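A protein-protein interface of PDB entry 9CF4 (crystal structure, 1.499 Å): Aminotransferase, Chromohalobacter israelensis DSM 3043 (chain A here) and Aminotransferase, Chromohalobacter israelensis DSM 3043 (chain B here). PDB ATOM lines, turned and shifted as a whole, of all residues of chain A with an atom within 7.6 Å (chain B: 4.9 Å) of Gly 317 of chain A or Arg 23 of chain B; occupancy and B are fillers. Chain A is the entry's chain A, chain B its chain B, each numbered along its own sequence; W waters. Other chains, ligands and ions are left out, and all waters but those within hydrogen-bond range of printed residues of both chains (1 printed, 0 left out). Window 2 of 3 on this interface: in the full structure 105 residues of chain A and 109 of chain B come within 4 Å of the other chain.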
ATOM      1  N   TYR A 132       0.609  15.391 -33.577  1.00  0.00           N
ATOM      2  CA  TYR A 132      -0.093  16.661 -33.712  1.00  0.00           C
ATOM      3  C   TYR A 132       0.885  17.818 -33.658  1.00  0.00           C
ATOM      4  O   TYR A 132       0.801  18.745 -34.477  1.00  0.00           O
ATOM      5  CB  TYR A 132      -1.105  16.746 -32.572  1.00  0.00           C
ATOM      6  CG  TYR A 132      -2.077  17.907 -32.600  1.00  0.00           C
ATOM      7  CD1 TYR A 132      -3.286  17.804 -33.248  1.00  0.00           C
ATOM      8  CD2 TYR A 132      -1.777  19.106 -31.965  1.00  0.00           C
ATOM      9  CE1 TYR A 132      -4.189  18.859 -33.271  1.00  0.00           C
ATOM     10  CE2 TYR A 132      -2.670  20.161 -31.977  1.00  0.00           C
ATOM     11  CZ  TYR A 132      -3.861  20.039 -32.627  1.00  0.00           C
ATOM     12  OH  TYR A 132      -4.738  21.089 -32.639  1.00  0.00           O
ATOM     13  N   TRP A 309       3.029  22.572 -25.012  1.00  0.00           N
ATOM     14  CA  TRP A 309       1.725  23.182 -24.755  1.00  0.00           C
ATOM     15  C   TRP A 309       1.488  24.374 -25.678  1.00  0.00           C
ATOM     16  O   TRP A 309       0.377  24.566 -26.186  1.00  0.00           O
ATOM     17  CB  TRP A 309       1.601  23.615 -23.294  1.00  0.00           C
ATOM     18  CG  TRP A 309       0.245  24.168 -23.063  1.00  0.00           C
ATOM     19  CD1 TRP A 309      -0.091  25.476 -22.846  1.00  0.00           C
ATOM     20  CD2 TRP A 309      -0.979  23.434 -23.080  1.00  0.00           C
ATOM     21  NE1 TRP A 309      -1.455  25.600 -22.731  1.00  0.00           N
ATOM     22  CE2 TRP A 309      -2.023  24.361 -22.883  1.00  0.00           C
ATOM     23  CE3 TRP A 309      -1.298  22.087 -23.265  1.00  0.00           C
ATOM     24  CZ2 TRP A 309      -3.353  23.976 -22.837  1.00  0.00           C
ATOM     25  CZ3 TRP A 309      -2.621  21.706 -23.241  1.00  0.00           C
ATOM     26  CH2 TRP A 309      -3.639  22.650 -23.016  1.00  0.00           C
ATOM     27  N   GLN A 310       2.501  25.170 -25.895  1.00  0.00           N
ATOM     28  CA  GLN A 310       2.358  26.320 -26.770  1.00  0.00           C
ATOM     29  C   GLN A 310       1.910  25.921 -28.164  1.00  0.00           C
ATOM     30  O   GLN A 310       1.111  26.553 -28.748  1.00  0.00           O
ATOM     31  CB  GLN A 310       3.645  27.129 -26.825  1.00  0.00           C
ATOM     32  CG  GLN A 310       3.503  28.412 -27.606  1.00  0.00           C
ATOM     33  CD  GLN A 310       4.769  29.283 -27.494  1.00  0.00           C
ATOM     34  OE1 GLN A 310       5.691  28.954 -26.763  1.00  0.00           O
ATOM     35  NE2 GLN A 310       4.790  30.424 -28.205  1.00  0.00           N
ATOM     36  N   VAL A 311       2.437  24.831 -28.665  1.00  0.00           N
ATOM     37  CA  VAL A 311       2.063  24.351 -29.989  1.00  0.00           C
ATOM     38  C   VAL A 311       0.676  23.708 -29.968  1.00  0.00           C
ATOM     39  O   VAL A 311      -0.051  23.806 -30.955  1.00  0.00           O
ATOM     40  CB  VAL A 311       3.148  23.394 -30.512  1.00  0.00           C
ATOM     41  CG1 VAL A 311       2.725  22.746 -31.827  1.00  0.00           C
ATOM     42  CG2 VAL A 311       4.457  24.155 -30.709  1.00  0.00           C
ATOM     43  N   LEU A 312       0.280  23.072 -28.858  1.00  0.00           N
ATOM     44  CA  LEU A 312      -1.095  22.598 -28.734  1.00  0.00           C
ATOM     45  C   LEU A 312      -2.078  23.768 -28.762  1.00  0.00           C
ATOM     46  O   LEU A 312      -3.152  23.661 -29.358  1.00  0.00           O
ATOM     47  CB  LEU A 312      -1.262  21.760 -27.478  1.00  0.00           C
ATOM     48  CG  LEU A 312      -0.442  20.468 -27.452  1.00  0.00           C
ATOM     49  CD1 LEU A 312      -0.819  19.653 -26.214  1.00  0.00           C
ATOM     50  CD2 LEU A 312      -0.598  19.663 -28.706  1.00  0.00           C
ATOM     51  N   GLU A 313      -1.710  24.902 -28.155  1.00  0.00           N
ATOM     52  CA  GLU A 313      -2.544  26.092 -28.255  1.00  0.00           C
ATOM     53  C   GLU A 313      -2.602  26.584 -29.700  1.00  0.00           C
ATOM     54  O   GLU A 313      -3.672  26.944 -30.204  1.00  0.00           O
ATOM     55  CB  GLU A 313      -2.013  27.193 -27.340  1.00  0.00           C
ATOM     56  CG  GLU A 313      -2.239  26.927 -25.860  1.00  0.00           C
ATOM     57  CD  GLU A 313      -2.057  28.153 -24.981  1.00  0.00           C
ATOM     58  OE1 GLU A 313      -1.578  29.211 -25.472  1.00  0.00           O
ATOM     59  OE2 GLU A 313      -2.393  28.074 -23.784  1.00  0.00           O
ATOM     60  N   GLN A 314      -1.453  26.632 -30.373  1.00  0.00           N
ATOM     61  CA  GLN A 314      -1.438  27.076 -31.762  1.00  0.00           C
ATOM     62  C   GLN A 314      -2.307  26.188 -32.635  1.00  0.00           C
ATOM     63  O   GLN A 314      -3.052  26.681 -33.493  1.00  0.00           O
ATOM     64  CB  GLN A 314       0.005  27.090 -32.281  1.00  0.00           C
ATOM     65  CG  GLN A 314       0.138  27.436 -33.751  1.00  0.00           C
ATOM     66  CD  GLN A 314       1.566  27.296 -34.269  1.00  0.00           C
ATOM     67  OE1 GLN A 314       2.541  27.389 -33.502  1.00  0.00           O
ATOM     68  NE2 GLN A 314       1.700  27.076 -35.576  1.00  0.00           N
ATOM     69  N   GLY A 315      -2.190  24.872 -32.464  1.00  0.00           N
ATOM     70  CA  GLY A 315      -2.948  23.941 -33.285  1.00  0.00           C
ATOM     71  C   GLY A 315      -4.446  24.060 -33.069  1.00  0.00           C
ATOM     72  O   GLY A 315      -5.220  24.062 -34.029  1.00  0.00           O
ATOM     73  N   THR A 316      -4.879  24.153 -31.806  1.00  0.00           N
ATOM     74  CA  THR A 316      -6.317  24.275 -31.556  1.00  0.00           C
ATOM     75  C   THR A 316      -6.836  25.632 -32.019  1.00  0.00           C
ATOM     76  O   THR A 316      -7.979  25.736 -32.460  1.00  0.00           O
ATOM     77  CB  THR A 316      -6.674  23.990 -30.099  1.00  0.00           C
ATOM     78  OG1 THR A 316      -5.910  24.817 -29.211  1.00  0.00           O
ATOM     79  CG2 THR A 316      -6.448  22.507 -29.774  1.00  0.00           C
ATOM     80  N   GLY A 317      -5.998  26.670 -31.953  1.00  0.00           N
ATOM     81  CA  GLY A 317      -6.373  27.935 -32.550  1.00  0.00           C
ATOM     82  C   GLY A 317      -6.655  27.813 -34.034  1.00  0.00           C
ATOM     83  O   GLY A 317      -7.582  28.434 -34.541  1.00  0.00           O
ATOM     84  N   GLU A 318      -5.860  27.006 -34.744  1.00  0.00           N
ATOM     85  CA  GLU A 318      -6.032  26.841 -36.184  1.00  0.00           C
ATOM     86  C   GLU A 318      -7.144  25.848 -36.519  1.00  0.00           C
ATOM     87  O   GLU A 318      -7.877  26.047 -37.489  1.00  0.00           O
ATOM     88  CB  GLU A 318      -4.736  26.341 -36.835  1.00  0.00           C
ATOM     89  CG  GLU A 318      -3.584  27.326 -36.817  1.00  0.00           C
ATOM     90  CD  GLU A 318      -2.284  26.750 -37.371  1.00  0.00           C
ATOM     91  OE1 GLU A 318      -2.347  25.864 -38.248  1.00  0.00           O
ATOM     92  OE2 GLU A 318      -1.202  27.227 -36.936  1.00  0.00           O
ATOM     93  N   PHE A 319      -7.279  24.759 -35.750  1.00  0.00           N
ATOM     94  CA  PHE A 319      -8.089  23.621 -36.174  1.00  0.00           C
ATOM     95  C   PHE A 319      -9.273  23.308 -35.270  1.00  0.00           C
ATOM     96  O   PHE A 319     -10.096  22.463 -35.637  1.00  0.00           O
ATOM     97  CB  PHE A 319      -7.212  22.365 -36.304  1.00  0.00           C
ATOM     98  CG  PHE A 319      -6.095  22.503 -37.304  1.00  0.00           C
ATOM     99  CD1 PHE A 319      -6.354  22.812 -38.626  1.00  0.00           C
ATOM    100  CD2 PHE A 319      -4.784  22.299 -36.925  1.00  0.00           C
ATOM    101  CE1 PHE A 319      -5.325  22.917 -39.547  1.00  0.00           C
ATOM    102  CE2 PHE A 319      -3.751  22.415 -37.845  1.00  0.00           C
ATOM    103  CZ  PHE A 319      -4.024  22.732 -39.153  1.00  0.00           C
ATOM    104  N   GLY A 320      -9.373  23.940 -34.105  1.00  0.00           N
ATOM    105  CA  GLY A 320     -10.500  23.740 -33.233  1.00  0.00           C
ATOM    106  C   GLY A 320     -10.218  22.726 -32.140  1.00  0.00           C
ATOM    107  O   GLY A 320      -9.083  22.313 -31.930  1.00  0.00           O
ATOM    108  N   PRO A 321     -11.268  22.303 -31.431  1.00  0.00           N
ATOM    109  CA  PRO A 321     -11.081  21.397 -30.294  1.00  0.00           C
ATOM    110  C   PRO A 321     -10.291  20.151 -30.671  1.00  0.00           C
ATOM    111  O   PRO A 321     -10.457  19.583 -31.755  1.00  0.00           O
ATOM    112  CB  PRO A 321     -12.517  21.060 -29.883  1.00  0.00           C
ATOM    113  CG  PRO A 321     -13.317  22.251 -30.328  1.00  0.00           C
ATOM    114  CD  PRO A 321     -12.681  22.695 -31.611  1.00  0.00           C
ATOM    115  N   HIS B  21     -11.217  23.087 -26.934  1.00  0.00           N
ATOM    116  CA  HIS B  21     -10.450  24.105 -27.638  1.00  0.00           C
ATOM    117  C   HIS B  21      -9.354  24.568 -26.683  1.00  0.00           C
ATOM    118  O   HIS B  21      -9.563  25.462 -25.857  1.00  0.00           O
ATOM    119  CB  HIS B  21     -11.334  25.261 -28.072  1.00  0.00           C
ATOM    120  CG  HIS B  21     -10.693  26.129 -29.096  1.00  0.00           C
ATOM    121  ND1 HIS B  21      -9.481  26.747 -28.876  1.00  0.00           N
ATOM    122  CD2 HIS B  21     -11.075  26.467 -30.351  1.00  0.00           C
ATOM    123  CE1 HIS B  21      -9.159  27.447 -29.951  1.00  0.00           C
ATOM    124  NE2 HIS B  21     -10.107  27.290 -30.859  1.00  0.00           N
ATOM    125  N   LEU B  22      -8.191  23.925 -26.757  1.00  0.00           N
ATOM    126  CA  LEU B  22      -7.187  24.077 -25.706  1.00  0.00           C
ATOM    127  C   LEU B  22      -6.737  25.525 -25.565  1.00  0.00           C
ATOM    128  O   LEU B  22      -6.584  26.028 -24.446  1.00  0.00           O
ATOM    129  CB  LEU B  22      -6.014  23.136 -25.980  1.00  0.00           C
ATOM    130  CG  LEU B  22      -6.361  21.654 -26.018  1.00  0.00           C
ATOM    131  CD1 LEU B  22      -5.100  20.839 -26.238  1.00  0.00           C
ATOM    132  CD2 LEU B  22      -7.051  21.199 -24.727  1.00  0.00           C
ATOM    133  N   ARG B  23      -6.529  26.225 -26.687  1.00  0.00           N
ATOM    134  CA  ARG B  23      -6.114  27.625 -26.610  1.00  0.00           C
ATOM    135  C   ARG B  23      -7.190  28.478 -25.949  1.00  0.00           C
ATOM    136  O   ARG B  23      -6.915  29.242 -25.013  1.00  0.00           O
ATOM    137  CB  ARG B  23      -5.833  28.168 -28.011  1.00  0.00           C
ATOM    138  CG  ARG B  23      -5.293  29.585 -27.980  1.00  0.00           C
ATOM    139  CD  ARG B  23      -5.437  30.291 -29.312  1.00  0.00           C
ATOM    140  NE  ARG B  23      -6.837  30.444 -29.711  1.00  0.00           N
ATOM    141  CZ  ARG B  23      -7.225  30.947 -30.876  1.00  0.00           C
ATOM    142  NH1 ARG B  23      -6.310  31.348 -31.756  1.00  0.00           N
ATOM    143  NH2 ARG B  23      -8.522  31.044 -31.172  1.00  0.00           N
ATOM    144  N   ASP B  24      -8.424  28.405 -26.466  1.00  0.00           N
ATOM    145  CA  ASP B  24      -9.472  29.281 -25.952  1.00  0.00           C
ATOM    146  C   ASP B  24      -9.777  28.975 -24.490  1.00  0.00           C
ATOM    147  O   ASP B  24     -10.019  29.888 -23.695  1.00  0.00           O
ATOM    148  CB  ASP B  24     -10.730  29.155 -26.806  1.00  0.00           C
ATOM    149  CG  ASP B  24     -10.609  29.852 -28.152  1.00  0.00           C
ATOM    150  OD1 ASP B  24      -9.578  30.518 -28.416  1.00  0.00           O
ATOM    151  OD2 ASP B  24     -11.559  29.726 -28.951  1.00  0.00           O
ATOM    152  N   PHE B  25      -9.730  27.707 -24.100  1.00  0.00           N
ATOM    153  CA  PHE B  25      -9.986  27.395 -22.698  1.00  0.00           C
ATOM    154  C   PHE B  25      -8.881  27.942 -21.806  1.00  0.00           C
ATOM    155  O   PHE B  25      -9.160  28.538 -20.760  1.00  0.00           O
ATOM    156  CB  PHE B  25     -10.166  25.888 -22.492  1.00  0.00           C
ATOM    157  CG  PHE B  25     -10.603  25.539 -21.099  1.00  0.00           C
ATOM    158  CD1 PHE B  25     -11.886  25.834 -20.664  1.00  0.00           C
ATOM    159  CD2 PHE B  25      -9.726  24.934 -20.209  1.00  0.00           C
ATOM    160  CE1 PHE B  25     -12.282  25.533 -19.369  1.00  0.00           C
ATOM    161  CE2 PHE B  25     -10.111  24.636 -18.927  1.00  0.00           C
ATOM    162  CZ  PHE B  25     -11.390  24.939 -18.490  1.00  0.00           C
ATOM    163  N   ALA B  26      -7.621  27.758 -22.201  1.00  0.00           N
ATOM    164  CA  ALA B  26      -6.520  28.235 -21.370  1.00  0.00           C
ATOM    165  C   ALA B  26      -6.518  29.748 -21.262  1.00  0.00           C
ATOM    166  O   ALA B  26      -6.084  30.291 -20.245  1.00  0.00           O
ATOM    167  CB  ALA B  26      -5.187  27.763 -21.920  1.00  0.00           C
ATOM    168  N   HIS B  27      -7.009  30.438 -22.279  1.00  0.00           N
ATOM    169  CA  HIS B  27      -6.953  31.896 -22.322  1.00  0.00           C
ATOM    170  C   HIS B  27      -8.235  32.568 -21.875  1.00  0.00           C
ATOM    171  O   HIS B  27      -8.317  33.800 -21.921  1.00  0.00           O
ATOM    172  CB  HIS B  27      -6.566  32.388 -23.711  1.00  0.00           C
ATOM    173  CG  HIS B  27      -5.131  32.137 -24.057  1.00  0.00           C
ATOM    174  ND1 HIS B  27      -4.159  33.103 -23.929  1.00  0.00           N
ATOM    175  CD2 HIS B  27      -4.504  31.028 -24.509  1.00  0.00           C
ATOM    176  CE1 HIS B  27      -2.993  32.600 -24.304  1.00  0.00           C
ATOM    177  NE2 HIS B  27      -3.180  31.347 -24.669  1.00  0.00           N
HETATM  178  O   HOH W   1     -10.076  28.520 -33.537  1.00  0.00           O
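OG1 of Thr 316 of chain A is in hydrogen-bond range of N of Leu 22 of chain B, 3.5 Å away.
O of Thr 316 of chain A is in hydrogen-bond range of NE2 of His 21 of chain B.
OG1 of Thr 316 of chain A sits at hydrogen-bond distance from N of Arg 23 of chain B, 3.0 Å away.
A ring nitrogen (NE2) of His 27 of chain B is in hydrogen-bond range of the side-chain carboxylate (OE1) of Glu 313 of chain A, at 2.8 Å.
Printed residues of chain B within 4 Å of Trp 309 of chain A: Leu 22 (3.8 Å).
Leu 312 of chain A touches none of the printed residues of chain B.
Printed residues of chain B within 4 Å of Gly 317 of chain A: His 21 (3.8 Å) and Arg 23 (3.5 Å).
Of the printed residues of chain A, His 21 of chain B touches Thr 316 (3.1 Å), Gly 317 (3.8 Å) and Pro 321 (3.8 Å).
Arg 23 of chain B touches just these residues of chain A: Glu 313 (3.3 Å), Thr 316 (3.0 Å) and Gly 317 (3.5 Å).
Of the printed residues of chain A, Ala 26 of chain B touches Glu 313 (3.4 Å).
Printed residues of chain A within 4 Å of His 27 of chain B: Glu 313.
The nearest printed residue of chain B that does not touch Gly 317 of chain A is Asp 24 of chain B (5.8 Å).
The nearest printed residue of chain A that does not touch His 27 of chain B is Trp 309 of chain A (6.3 Å).
Printed residues of chain B that touch a printed residue of chain A: His 21, Leu 22, Arg 23, Ala 26 and His 27.
Hydrophobic or aromatic side chains of chain B within 4 Å of the printed part of chain A: His 21, Leu 22, Ala 26 and His 27.
Hydrophobic or aromatic side chains of chain A within 4 Å of the printed part of chain B: Trp 309 and Pro 321.
Among the printed residues, no Asp or Glu carboxylate lies within 4 Å of a Lys or Arg side-chain nitrogen of the other chain.
The side-chain hydroxyl of Tyr 132 of chain A is in hydrogen-bond range of the backbone NH of Thr 316 of chain A (3.2 Å).
A ring nitrogen (ND1) of His 21 of chain B lies within hydrogen-bond range of the backbone NH (N) of Asp 24 of chain B, at 3.1 Å.
The indole nitrogen (NE1) of Trp 309 of chain A sits at hydrogen-bond distance from the side-chain carboxylate (OE2) of Glu 313 of chain A.
The guanidinium group (NH2) of Arg 23 of chain B lies within salt-bridge range of the side-chain carboxylate (OD1) of Asp 24 of chain B (3.0 Å).
The backbone carbonyl oxygen (O) of Leu 312 of chain A is in hydrogen-bond range of the side-chain hydroxyl (OG1) of Thr 316 of chain A (3.0 Å).
The side-chain hydroxyl (OG1) of Thr 316 of chain A is in hydrogen-bond range of the backbone carbonyl oxygen (O) of Glu 313 of chain A, 3.2 Å away.
Water W1 bridges the backbone carbonyl oxygen of Gly 317 of chain A (2.7 Å) and a ring nitrogen (NE2) of His 21 of chain B (2.9 Å).
Leu 22 of chain B touches Trp 309 of chain A.
CB of Arg 23 of chain B touches O of Glu 313 of chain A, 3.3 Å away.
OE2 of Glu 313 of chain A touches CB of Ala 26 of chain B, at 3.4 Å.
His 21 of chain B touches Gly 317 of chain A.
CA of Gly 317 of chain A touches NH1 of Arg 23 of chain B, at 3.5 Å.
N of His 21 of chain B touches CA of Pro 321 of chain A (3.8 Å).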
